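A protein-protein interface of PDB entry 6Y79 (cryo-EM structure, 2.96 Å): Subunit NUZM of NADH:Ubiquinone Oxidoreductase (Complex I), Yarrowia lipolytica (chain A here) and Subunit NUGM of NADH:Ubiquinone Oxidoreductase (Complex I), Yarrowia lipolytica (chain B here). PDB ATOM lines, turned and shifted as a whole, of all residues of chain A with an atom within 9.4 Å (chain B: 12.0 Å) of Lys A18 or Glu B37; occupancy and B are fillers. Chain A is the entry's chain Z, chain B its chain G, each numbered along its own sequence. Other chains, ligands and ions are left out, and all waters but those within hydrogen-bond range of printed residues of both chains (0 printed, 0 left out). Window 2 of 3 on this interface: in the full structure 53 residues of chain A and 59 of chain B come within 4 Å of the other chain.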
ATOM      1  N   VAL A   9     -13.143  36.228  16.159  1.00  0.00           N
ATOM      2  CA  VAL A   9     -14.321  35.451  15.789  1.00  0.00           C
ATOM      3  C   VAL A   9     -13.902  34.154  15.093  1.00  0.00           C
ATOM      4  O   VAL A   9     -14.059  33.954  13.881  1.00  0.00           O
ATOM      5  CB  VAL A   9     -15.343  36.323  15.010  1.00  0.00           C
ATOM      6  CG1 VAL A   9     -14.779  36.996  13.721  1.00  0.00           C
ATOM      7  CG2 VAL A   9     -16.652  35.554  14.773  1.00  0.00           C
ATOM      8  N   PHE A  10     -13.397  33.231  15.902  1.00  0.00           N
ATOM      9  CA  PHE A  10     -13.419  31.813  15.588  1.00  0.00           C
ATOM     10  C   PHE A  10     -13.658  31.024  16.865  1.00  0.00           C
ATOM     11  O   PHE A  10     -13.588  29.789  16.841  1.00  0.00           O
ATOM     12  CB  PHE A  10     -12.136  31.348  14.854  1.00  0.00           C
ATOM     13  CG  PHE A  10     -10.857  31.498  15.635  1.00  0.00           C
ATOM     14  CD1 PHE A  10     -10.085  32.636  15.505  1.00  0.00           C
ATOM     15  CD2 PHE A  10     -10.387  30.468  16.434  1.00  0.00           C
ATOM     16  CE1 PHE A  10      -8.891  32.761  16.192  1.00  0.00           C
ATOM     17  CE2 PHE A  10      -9.198  30.595  17.132  1.00  0.00           C
ATOM     18  CZ  PHE A  10      -8.453  31.741  17.008  1.00  0.00           C
ATOM     19  N   TYR A  13     -18.949  30.670  17.782  1.00  0.00           N
ATOM     20  CA  TYR A  13     -20.043  29.738  17.456  1.00  0.00           C
ATOM     21  C   TYR A  13     -21.149  30.402  16.636  1.00  0.00           C
ATOM     22  O   TYR A  13     -22.312  30.450  17.035  1.00  0.00           O
ATOM     23  CB  TYR A  13     -20.623  29.096  18.719  1.00  0.00           C
ATOM     24  CG  TYR A  13     -19.647  28.201  19.420  1.00  0.00           C
ATOM     25  CD1 TYR A  13     -19.443  26.907  18.983  1.00  0.00           C
ATOM     26  CD2 TYR A  13     -18.915  28.655  20.500  1.00  0.00           C
ATOM     27  CE1 TYR A  13     -18.546  26.083  19.607  1.00  0.00           C
ATOM     28  CE2 TYR A  13     -18.013  27.840  21.132  1.00  0.00           C
ATOM     29  CZ  TYR A  13     -17.832  26.555  20.679  1.00  0.00           C
ATOM     30  OH  TYR A  13     -16.931  25.735  21.310  1.00  0.00           O
ATOM     31  N   THR A  14     -20.756  30.921  15.478  1.00  0.00           N
ATOM     32  CA  THR A  14     -21.632  31.686  14.608  1.00  0.00           C
ATOM     33  C   THR A  14     -21.075  31.549  13.194  1.00  0.00           C
ATOM     34  O   THR A  14     -19.858  31.526  13.005  1.00  0.00           O
ATOM     35  CB  THR A  14     -21.720  33.149  15.103  1.00  0.00           C
ATOM     36  OG1 THR A  14     -22.265  33.191  16.425  1.00  0.00           O
ATOM     37  CG2 THR A  14     -22.611  33.947  14.265  1.00  0.00           C
ATOM     38  N   VAL A  15     -21.974  31.464  12.204  1.00  0.00           N
ATOM     39  CA  VAL A  15     -21.654  30.925  10.877  1.00  0.00           C
ATOM     40  C   VAL A  15     -20.629  31.764  10.102  1.00  0.00           C
ATOM     41  O   VAL A  15     -19.843  31.196   9.344  1.00  0.00           O
ATOM     42  CB  VAL A  15     -22.994  30.701  10.129  1.00  0.00           C
ATOM     43  CG1 VAL A  15     -22.833  30.506   8.623  1.00  0.00           C
ATOM     44  CG2 VAL A  15     -23.700  29.493  10.711  1.00  0.00           C
ATOM     45  N   GLY A  16     -20.551  33.069  10.321  1.00  0.00           N
ATOM     46  CA  GLY A  16     -19.392  33.819   9.843  1.00  0.00           C
ATOM     47  C   GLY A  16     -19.279  33.908   8.324  1.00  0.00           C
ATOM     48  O   GLY A  16     -20.210  34.351   7.642  1.00  0.00           O
ATOM     49  N   SER A  17     -18.140  33.449   7.789  1.00  0.00           N
ATOM     50  CA  SER A  17     -17.837  33.491   6.359  1.00  0.00           C
ATOM     51  C   SER A  17     -16.626  32.624   6.040  1.00  0.00           C
ATOM     52  O   SER A  17     -15.823  32.296   6.918  1.00  0.00           O
ATOM     53  CB  SER A  17     -17.556  34.910   5.889  1.00  0.00           C
ATOM     54  OG  SER A  17     -16.381  35.375   6.485  1.00  0.00           O
ATOM     55  N   LYS A  18     -16.467  32.323   4.751  1.00  0.00           N
ATOM     56  CA  LYS A  18     -15.371  31.484   4.281  1.00  0.00           C
ATOM     57  C   LYS A  18     -14.863  31.988   2.933  1.00  0.00           C
ATOM     58  O   LYS A  18     -15.599  32.631   2.181  1.00  0.00           O
ATOM     59  CB  LYS A  18     -15.803  30.019   4.151  1.00  0.00           C
ATOM     60  CG  LYS A  18     -16.879  29.809   3.103  1.00  0.00           C
ATOM     61  CD  LYS A  18     -17.248  28.356   2.960  1.00  0.00           C
ATOM     62  CE  LYS A  18     -17.996  27.919   4.202  1.00  0.00           C
ATOM     63  NZ  LYS A  18     -18.578  26.551   4.195  1.00  0.00           N
ATOM     64  N   GLY A  19     -13.597  31.697   2.642  1.00  0.00           N
ATOM     65  CA  GLY A  19     -13.019  32.024   1.354  1.00  0.00           C
ATOM     66  C   GLY A  19     -12.311  33.360   1.328  1.00  0.00           C
ATOM     67  O   GLY A  19     -11.746  33.786   2.339  1.00  0.00           O
ATOM     68  N   ILE A  20     -12.319  34.029   0.171  1.00  0.00           N
ATOM     69  CA  ILE A  20     -11.768  35.376   0.096  1.00  0.00           C
ATOM     70  C   ILE A  20     -12.818  36.417   0.443  1.00  0.00           C
ATOM     71  O   ILE A  20     -12.504  37.613   0.521  1.00  0.00           O
ATOM     72  CB  ILE A  20     -11.152  35.651  -1.291  1.00  0.00           C
ATOM     73  CG1 ILE A  20     -12.200  35.577  -2.400  1.00  0.00           C
ATOM     74  CG2 ILE A  20     -10.013  34.687  -1.565  1.00  0.00           C
ATOM     75  CD1 ILE A  20     -11.673  36.037  -3.754  1.00  0.00           C
ATOM     76  N   TRP A  21     -14.062  35.988   0.672  1.00  0.00           N
ATOM     77  CA  TRP A  21     -15.073  36.898   1.188  1.00  0.00           C
ATOM     78  C   TRP A  21     -14.762  37.307   2.619  1.00  0.00           C
ATOM     79  O   TRP A  21     -15.103  38.422   3.034  1.00  0.00           O
ATOM     80  CB  TRP A  21     -16.455  36.257   1.080  1.00  0.00           C
ATOM     81  CG  TRP A  21     -16.833  36.027  -0.337  1.00  0.00           C
ATOM     82  CD1 TRP A  21     -16.906  34.833  -0.985  1.00  0.00           C
ATOM     83  CD2 TRP A  21     -17.148  37.030  -1.304  1.00  0.00           C
ATOM     84  NE1 TRP A  21     -17.269  35.029  -2.295  1.00  0.00           N
ATOM     85  CE2 TRP A  21     -17.416  36.372  -2.517  1.00  0.00           C
ATOM     86  CE3 TRP A  21     -17.236  38.422  -1.261  1.00  0.00           C
ATOM     87  CZ2 TRP A  21     -17.772  37.056  -3.670  1.00  0.00           C
ATOM     88  CZ3 TRP A  21     -17.584  39.097  -2.406  1.00  0.00           C
ATOM     89  CH2 TRP A  21     -17.847  38.417  -3.591  1.00  0.00           C
ATOM     90  N   GLU A  22     -14.056  36.459   3.367  1.00  0.00           N
ATOM     91  CA  GLU A  22     -13.632  36.881   4.694  1.00  0.00           C
ATOM     92  C   GLU A  22     -12.463  37.853   4.606  1.00  0.00           C
ATOM     93  O   GLU A  22     -12.361  38.786   5.413  1.00  0.00           O
ATOM     94  CB  GLU A  22     -13.297  35.669   5.547  1.00  0.00           C
ATOM     95  CG  GLU A  22     -13.264  35.929   7.043  1.00  0.00           C
ATOM     96  CD  GLU A  22     -11.860  36.143   7.548  1.00  0.00           C
ATOM     97  OE1 GLU A  22     -10.959  35.746   6.807  1.00  0.00           O
ATOM     98  OE2 GLU A  22     -11.684  36.629   8.683  1.00  0.00           O
ATOM     99  N   LYS A  23     -11.617  37.704   3.586  1.00  0.00           N
ATOM    100  CA  LYS A  23     -10.552  38.675   3.367  1.00  0.00           C
ATOM    101  C   LYS A  23     -11.107  40.002   2.882  1.00  0.00           C
ATOM    102  O   LYS A  23     -10.477  41.047   3.073  1.00  0.00           O
ATOM    103  CB  LYS A  23      -9.518  38.117   2.385  1.00  0.00           C
ATOM    104  CG  LYS A  23      -8.742  36.886   2.886  1.00  0.00           C
ATOM    105  CD  LYS A  23      -7.751  37.232   4.020  1.00  0.00           C
ATOM    106  CE  LYS A  23      -8.243  36.778   5.404  1.00  0.00           C
ATOM    107  NZ  LYS A  23      -7.351  37.128   6.551  1.00  0.00           N
ATOM    108  N   LEU A  24     -12.284  39.981   2.270  1.00  0.00           N
ATOM    109  CA  LEU A  24     -12.944  41.231   1.930  1.00  0.00           C
ATOM    110  C   LEU A  24     -13.613  41.850   3.152  1.00  0.00           C
ATOM    111  O   LEU A  24     -13.618  43.074   3.314  1.00  0.00           O
ATOM    112  CB  LEU A  24     -13.946  40.986   0.812  1.00  0.00           C
ATOM    113  CG  LEU A  24     -14.800  42.168   0.381  1.00  0.00           C
ATOM    114  CD1 LEU A  24     -13.957  43.250  -0.256  1.00  0.00           C
ATOM    115  CD2 LEU A  24     -15.754  41.644  -0.615  1.00  0.00           C
ATOM    116  N   ARG A  25     -14.185  41.035   4.033  1.00  0.00           N
ATOM    117  CA  ARG A  25     -14.914  41.652   5.135  1.00  0.00           C
ATOM    118  C   ARG A  25     -14.038  42.012   6.325  1.00  0.00           C
ATOM    119  O   ARG A  25     -14.536  42.659   7.248  1.00  0.00           O
ATOM    120  CB  ARG A  25     -16.028  40.753   5.619  1.00  0.00           C
ATOM    121  CG  ARG A  25     -15.479  39.555   6.270  1.00  0.00           C
ATOM    122  CD  ARG A  25     -16.569  38.624   6.676  1.00  0.00           C
ATOM    123  NE  ARG A  25     -17.306  39.122   7.820  1.00  0.00           N
ATOM    124  CZ  ARG A  25     -16.911  38.949   9.076  1.00  0.00           C
ATOM    125  NH1 ARG A  25     -15.783  38.297   9.337  1.00  0.00           N
ATOM    126  NH2 ARG A  25     -17.644  39.420  10.077  1.00  0.00           N
ATOM    127  N   ILE A  40     -24.422  28.198  14.536  1.00  0.00           N
ATOM    128  CA  ILE A  40     -23.924  27.101  13.712  1.00  0.00           C
ATOM    129  C   ILE A  40     -24.874  25.918  13.833  1.00  0.00           C
ATOM    130  O   ILE A  40     -25.041  25.357  14.920  1.00  0.00           O
ATOM    131  CB  ILE A  40     -22.500  26.703  14.118  1.00  0.00           C
ATOM    132  CG1 ILE A  40     -21.545  27.877  13.929  1.00  0.00           C
ATOM    133  CG2 ILE A  40     -22.029  25.532  13.288  1.00  0.00           C
ATOM    134  CD1 ILE A  40     -20.143  27.590  14.380  1.00  0.00           C
ATOM    135  N   PRO A  42     -24.984  22.541  12.770  1.00  0.00           N
ATOM    136  CA  PRO A  42     -24.647  21.242  13.380  1.00  0.00           C
ATOM    137  C   PRO A  42     -24.308  21.303  14.862  1.00  0.00           C
ATOM    138  O   PRO A  42     -24.320  20.256  15.517  1.00  0.00           O
ATOM    139  CB  PRO A  42     -23.437  20.772  12.561  1.00  0.00           C
ATOM    140  CG  PRO A  42     -22.843  22.005  12.056  1.00  0.00           C
ATOM    141  CD  PRO A  42     -24.023  22.821  11.679  1.00  0.00           C
ATOM    142  N   LEU A  43     -24.019  22.480  15.418  1.00  0.00           N
ATOM    143  CA  LEU A  43     -23.676  22.608  16.829  1.00  0.00           C
ATOM    144  C   LEU A  43     -24.878  23.025  17.669  1.00  0.00           C
ATOM    145  O   LEU A  43     -25.233  22.345  18.634  1.00  0.00           O
ATOM    146  CB  LEU A  43     -22.543  23.624  17.013  1.00  0.00           C
ATOM    147  CG  LEU A  43     -21.261  23.383  16.221  1.00  0.00           C
ATOM    148  CD1 LEU A  43     -20.264  24.504  16.473  1.00  0.00           C
ATOM    149  CD2 LEU A  43     -20.660  22.001  16.525  1.00  0.00           C
ATOM    150  N   PRO B  34      -9.073  28.752  12.720  1.00  0.00           N
ATOM    151  CA  PRO B  34      -9.404  30.165  12.529  1.00  0.00           C
ATOM    152  C   PRO B  34     -10.691  30.277  11.732  1.00  0.00           C
ATOM    153  O   PRO B  34     -10.945  31.280  11.048  1.00  0.00           O
ATOM    154  CB  PRO B  34      -8.219  30.695  11.739  1.00  0.00           C
ATOM    155  CG  PRO B  34      -7.738  29.508  10.963  1.00  0.00           C
ATOM    156  CD  PRO B  34      -7.935  28.329  11.885  1.00  0.00           C
ATOM    157  N   SER B  35     -11.491  29.226  11.820  1.00  0.00           N
ATOM    158  CA  SER B  35     -12.613  29.017  10.929  1.00  0.00           C
ATOM    159  C   SER B  35     -13.823  28.597  11.753  1.00  0.00           C
ATOM    160  O   SER B  35     -13.721  28.270  12.943  1.00  0.00           O
ATOM    161  CB  SER B  35     -12.255  27.971   9.856  1.00  0.00           C
ATOM    162  OG  SER B  35     -11.228  28.430   9.029  1.00  0.00           O
ATOM    163  N   TRP B  36     -14.986  28.630  11.118  1.00  0.00           N
ATOM    164  CA  TRP B  36     -16.192  28.138  11.763  1.00  0.00           C
ATOM    165  C   TRP B  36     -16.501  26.701  11.381  1.00  0.00           C
ATOM    166  O   TRP B  36     -17.448  26.114  11.909  1.00  0.00           O
ATOM    167  CB  TRP B  36     -17.372  29.042  11.432  1.00  0.00           C
ATOM    168  CG  TRP B  36     -17.788  29.026  10.001  1.00  0.00           C
ATOM    169  CD1 TRP B  36     -17.224  29.718   8.974  1.00  0.00           C
ATOM    170  CD2 TRP B  36     -18.880  28.291   9.439  1.00  0.00           C
ATOM    171  NE1 TRP B  36     -17.897  29.463   7.804  1.00  0.00           N
ATOM    172  CE2 TRP B  36     -18.915  28.583   8.063  1.00  0.00           C
ATOM    173  CE3 TRP B  36     -19.836  27.417   9.969  1.00  0.00           C
ATOM    174  CZ2 TRP B  36     -19.871  28.035   7.210  1.00  0.00           C
ATOM    175  CZ3 TRP B  36     -20.776  26.865   9.116  1.00  0.00           C
ATOM    176  CH2 TRP B  36     -20.787  27.177   7.751  1.00  0.00           C
ATOM    177  N   GLU B  37     -15.715  26.136  10.472  1.00  0.00           N
ATOM    178  CA  GLU B  37     -15.700  24.723  10.138  1.00  0.00           C
ATOM    179  C   GLU B  37     -14.932  23.939  11.184  1.00  0.00           C
ATOM    180  O   GLU B  37     -15.348  22.843  11.587  1.00  0.00           O
ATOM    181  CB  GLU B  37     -15.006  24.523   8.786  1.00  0.00           C
ATOM    182  CG  GLU B  37     -15.650  25.118   7.540  1.00  0.00           C
ATOM    183  CD  GLU B  37     -15.478  26.666   7.375  1.00  0.00           C
ATOM    184  OE1 GLU B  37     -15.132  27.366   8.361  1.00  0.00           O
ATOM    185  OE2 GLU B  37     -15.629  27.110   6.242  1.00  0.00           O
ATOM    186  N   ASN B  38     -13.803  24.494  11.604  1.00  0.00           N
ATOM    187  CA  ASN B  38     -12.815  23.854  12.452  1.00  0.00           C
ATOM    188  C   ASN B  38     -12.971  24.233  13.917  1.00  0.00           C
ATOM    189  O   ASN B  38     -12.066  23.967  14.715  1.00  0.00           O
ATOM    190  CB  ASN B  38     -11.417  24.202  11.934  1.00  0.00           C
ATOM    191  CG  ASN B  38     -11.209  23.749  10.492  1.00  0.00           C
ATOM    192  OD1 ASN B  38     -10.845  22.603  10.243  1.00  0.00           O
ATOM    193  ND2 ASN B  38     -11.459  24.641   9.538  1.00  0.00           N
ATOM    194  N   ILE B  39     -14.096  24.851  14.279  1.00  0.00           N
ATOM    195  CA  ILE B  39     -14.382  25.151  15.673  1.00  0.00           C
ATOM    196  C   ILE B  39     -14.712  23.856  16.404  1.00  0.00           C
ATOM    197  O   ILE B  39     -15.289  22.917  15.833  1.00  0.00           O
ATOM    198  CB  ILE B  39     -15.511  26.197  15.775  1.00  0.00           C
ATOM    199  CG1 ILE B  39     -15.621  26.764  17.190  1.00  0.00           C
ATOM    200  CG2 ILE B  39     -16.858  25.658  15.289  1.00  0.00           C
ATOM    201  CD1 ILE B  39     -16.408  28.041  17.268  1.00  0.00           C
ATOM    202  N   LYS B  40     -14.274  23.768  17.655  1.00  0.00           N
ATOM    203  CA  LYS B  40     -14.538  22.574  18.434  1.00  0.00           C
ATOM    204  C   LYS B  40     -15.989  22.549  18.897  1.00  0.00           C
ATOM    205  O   LYS B  40     -16.615  23.586  19.127  1.00  0.00           O
ATOM    206  CB  LYS B  40     -13.595  22.492  19.635  1.00  0.00           C
ATOM    207  CG  LYS B  40     -13.707  23.649  20.606  1.00  0.00           C
ATOM    208  CD  LYS B  40     -12.701  23.527  21.732  1.00  0.00           C
ATOM    209  CE  LYS B  40     -13.014  22.337  22.624  1.00  0.00           C
ATOM    210  NZ  LYS B  40     -14.299  22.498  23.354  1.00  0.00           N
ATOM    211  N   ASP B  41     -16.528  21.343  18.997  1.00  0.00           N
ATOM    212  CA  ASP B  41     -17.794  21.115  19.665  1.00  0.00           C
ATOM    213  C   ASP B  41     -17.563  21.042  21.164  1.00  0.00           C
ATOM    214  O   ASP B  41     -16.482  20.668  21.626  1.00  0.00           O
ATOM    215  CB  ASP B  41     -18.435  19.823  19.178  1.00  0.00           C
ATOM    216  CG  ASP B  41     -19.928  19.875  19.226  1.00  0.00           C
ATOM    217  OD1 ASP B  41     -20.473  20.856  19.778  1.00  0.00           O
ATOM    218  OD2 ASP B  41     -20.569  18.938  18.701  1.00  0.00           O
ATOM    219  N   ILE B  42     -18.591  21.389  21.929  1.00  0.00           N
ATOM    220  CA  ILE B  42     -18.482  21.244  23.373  1.00  0.00           C
ATOM    221  C   ILE B  42     -19.395  20.149  23.902  1.00  0.00           C
ATOM    222  O   ILE B  42     -19.335  19.822  25.089  1.00  0.00           O
ATOM    223  CB  ILE B  42     -18.760  22.578  24.077  1.00  0.00           C
ATOM    224  CG1 ILE B  42     -20.150  23.085  23.717  1.00  0.00           C
ATOM    225  CG2 ILE B  42     -17.715  23.609  23.716  1.00  0.00           C
ATOM    226  CD1 ILE B  42     -20.504  24.327  24.460  1.00  0.00           C
ATOM    227  N   ARG B  43     -20.259  19.592  23.053  1.00  0.00           N
ATOM    228  CA  ARG B  43     -21.057  18.443  23.461  1.00  0.00           C
ATOM    229  C   ARG B  43     -20.188  17.209  23.680  1.00  0.00           C
ATOM    230  O   ARG B  43     -20.492  16.387  24.549  1.00  0.00           O
ATOM    231  CB  ARG B  43     -22.133  18.169  22.418  1.00  0.00           C
ATOM    232  CG  ARG B  43     -22.832  19.425  21.968  1.00  0.00           C
ATOM    233  CD  ARG B  43     -23.823  19.137  20.865  1.00  0.00           C
ATOM    234  NE  ARG B  43     -23.159  18.933  19.586  1.00  0.00           N
ATOM    235  CZ  ARG B  43     -23.628  18.161  18.616  1.00  0.00           C
ATOM    236  NH1 ARG B  43     -22.954  18.037  17.487  1.00  0.00           N
ATOM    237  NH2 ARG B  43     -24.763  17.506  18.777  1.00  0.00           N
ATOM    238  N   LEU B  44     -19.106  17.069  22.911  1.00  0.00           N
ATOM    239  CA  LEU B  44     -18.099  16.032  23.126  1.00  0.00           C
ATOM    240  C   LEU B  44     -17.047  16.612  24.050  1.00  0.00           C
ATOM    241  O   LEU B  44     -16.143  17.331  23.614  1.00  0.00           O
ATOM    242  CB  LEU B  44     -17.461  15.579  21.821  1.00  0.00           C
ATOM    243  CG  LEU B  44     -18.233  14.820  20.751  1.00  0.00           C
ATOM    244  CD1 LEU B  44     -17.324  14.657  19.547  1.00  0.00           C
ATOM    245  CD2 LEU B  44     -18.737  13.462  21.243  1.00  0.00           C
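O of Lys B40 is in hydrogen-bond range of OH of Tyr A13, at 3.1 Å. NE1 of Trp B36 is in hydrogen-bond range of O of Val A15, at 3.0 Å. The side-chain carboxylate (OE2) of Glu B37 lies within salt-bridge range of the side-chain amino group (NZ) of Lys A18. NH1 of Arg B43 lies within hydrogen-bond range of O of Pro A42, 3.3 Å away.
NE of Arg B43 is in salt-bridge range of OD2 of Asp B41 (2.7 Å).
Phe A10 touches Pro B34. CB of Phe A10 touches N of Ser B35, at 3.8 Å. CD1 of Ile B39 touches O of Phe A10 (3.3 Å). Ile B39 touches Tyr A13 (CD1 to CD1, 3.7 Å). Ile B42 touches Tyr A13. Thr A14 touches Trp B36 (O to CB, 3.9 Å). Trp B36 touches Lys A18 (CZ2 to CE, 3.5 Å). Ile A40 touches Trp B36. Ile A40 touches Ile B39. Asp B41 touches Leu A43.
No residue of chain B comes within 4 Å of Gly A16. No residue of chain B comes within 4 Å of Ile A20. No residue of chain B comes within 4 Å of Glu A22. Leu A24 touches none of the printed residues of chain B. Of the printed residues of chain B, Leu A43 touches Ile B39 (3.8 Å) and Asp B41 (3.5 Å). Of chain A, only Thr A14, Val A15, Ser A17, Lys A18 and Ile A40 come within 4 Å of Trp B36. Glu B37 touches just one residue of chain A: Lys A18 (3.2 Å). Of the printed residues of chain A, Ile B42 touches Tyr A13. The nearest residue of chain B that does not touch Lys A18 is Ser B35 (6.9 Å). The nearest printed residue of chain B that does not touch Ile A40 is Glu B37 (6.1 Å).
Of the 11 printed residues of chain B, 9 touch a printed residue of chain A. Hydrophobic or aromatic side chains of chain B within 4 Å of the printed part of chain A: Trp B36, Ile B39 and Ile B42. Among the printed residues, 16 pairs touch across the chains. Among the printed residues, Asp or Glu carboxylates within 4 Å of a Lys or Arg side-chain nitrogen of the other chain: Lys A18 with Glu B37.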
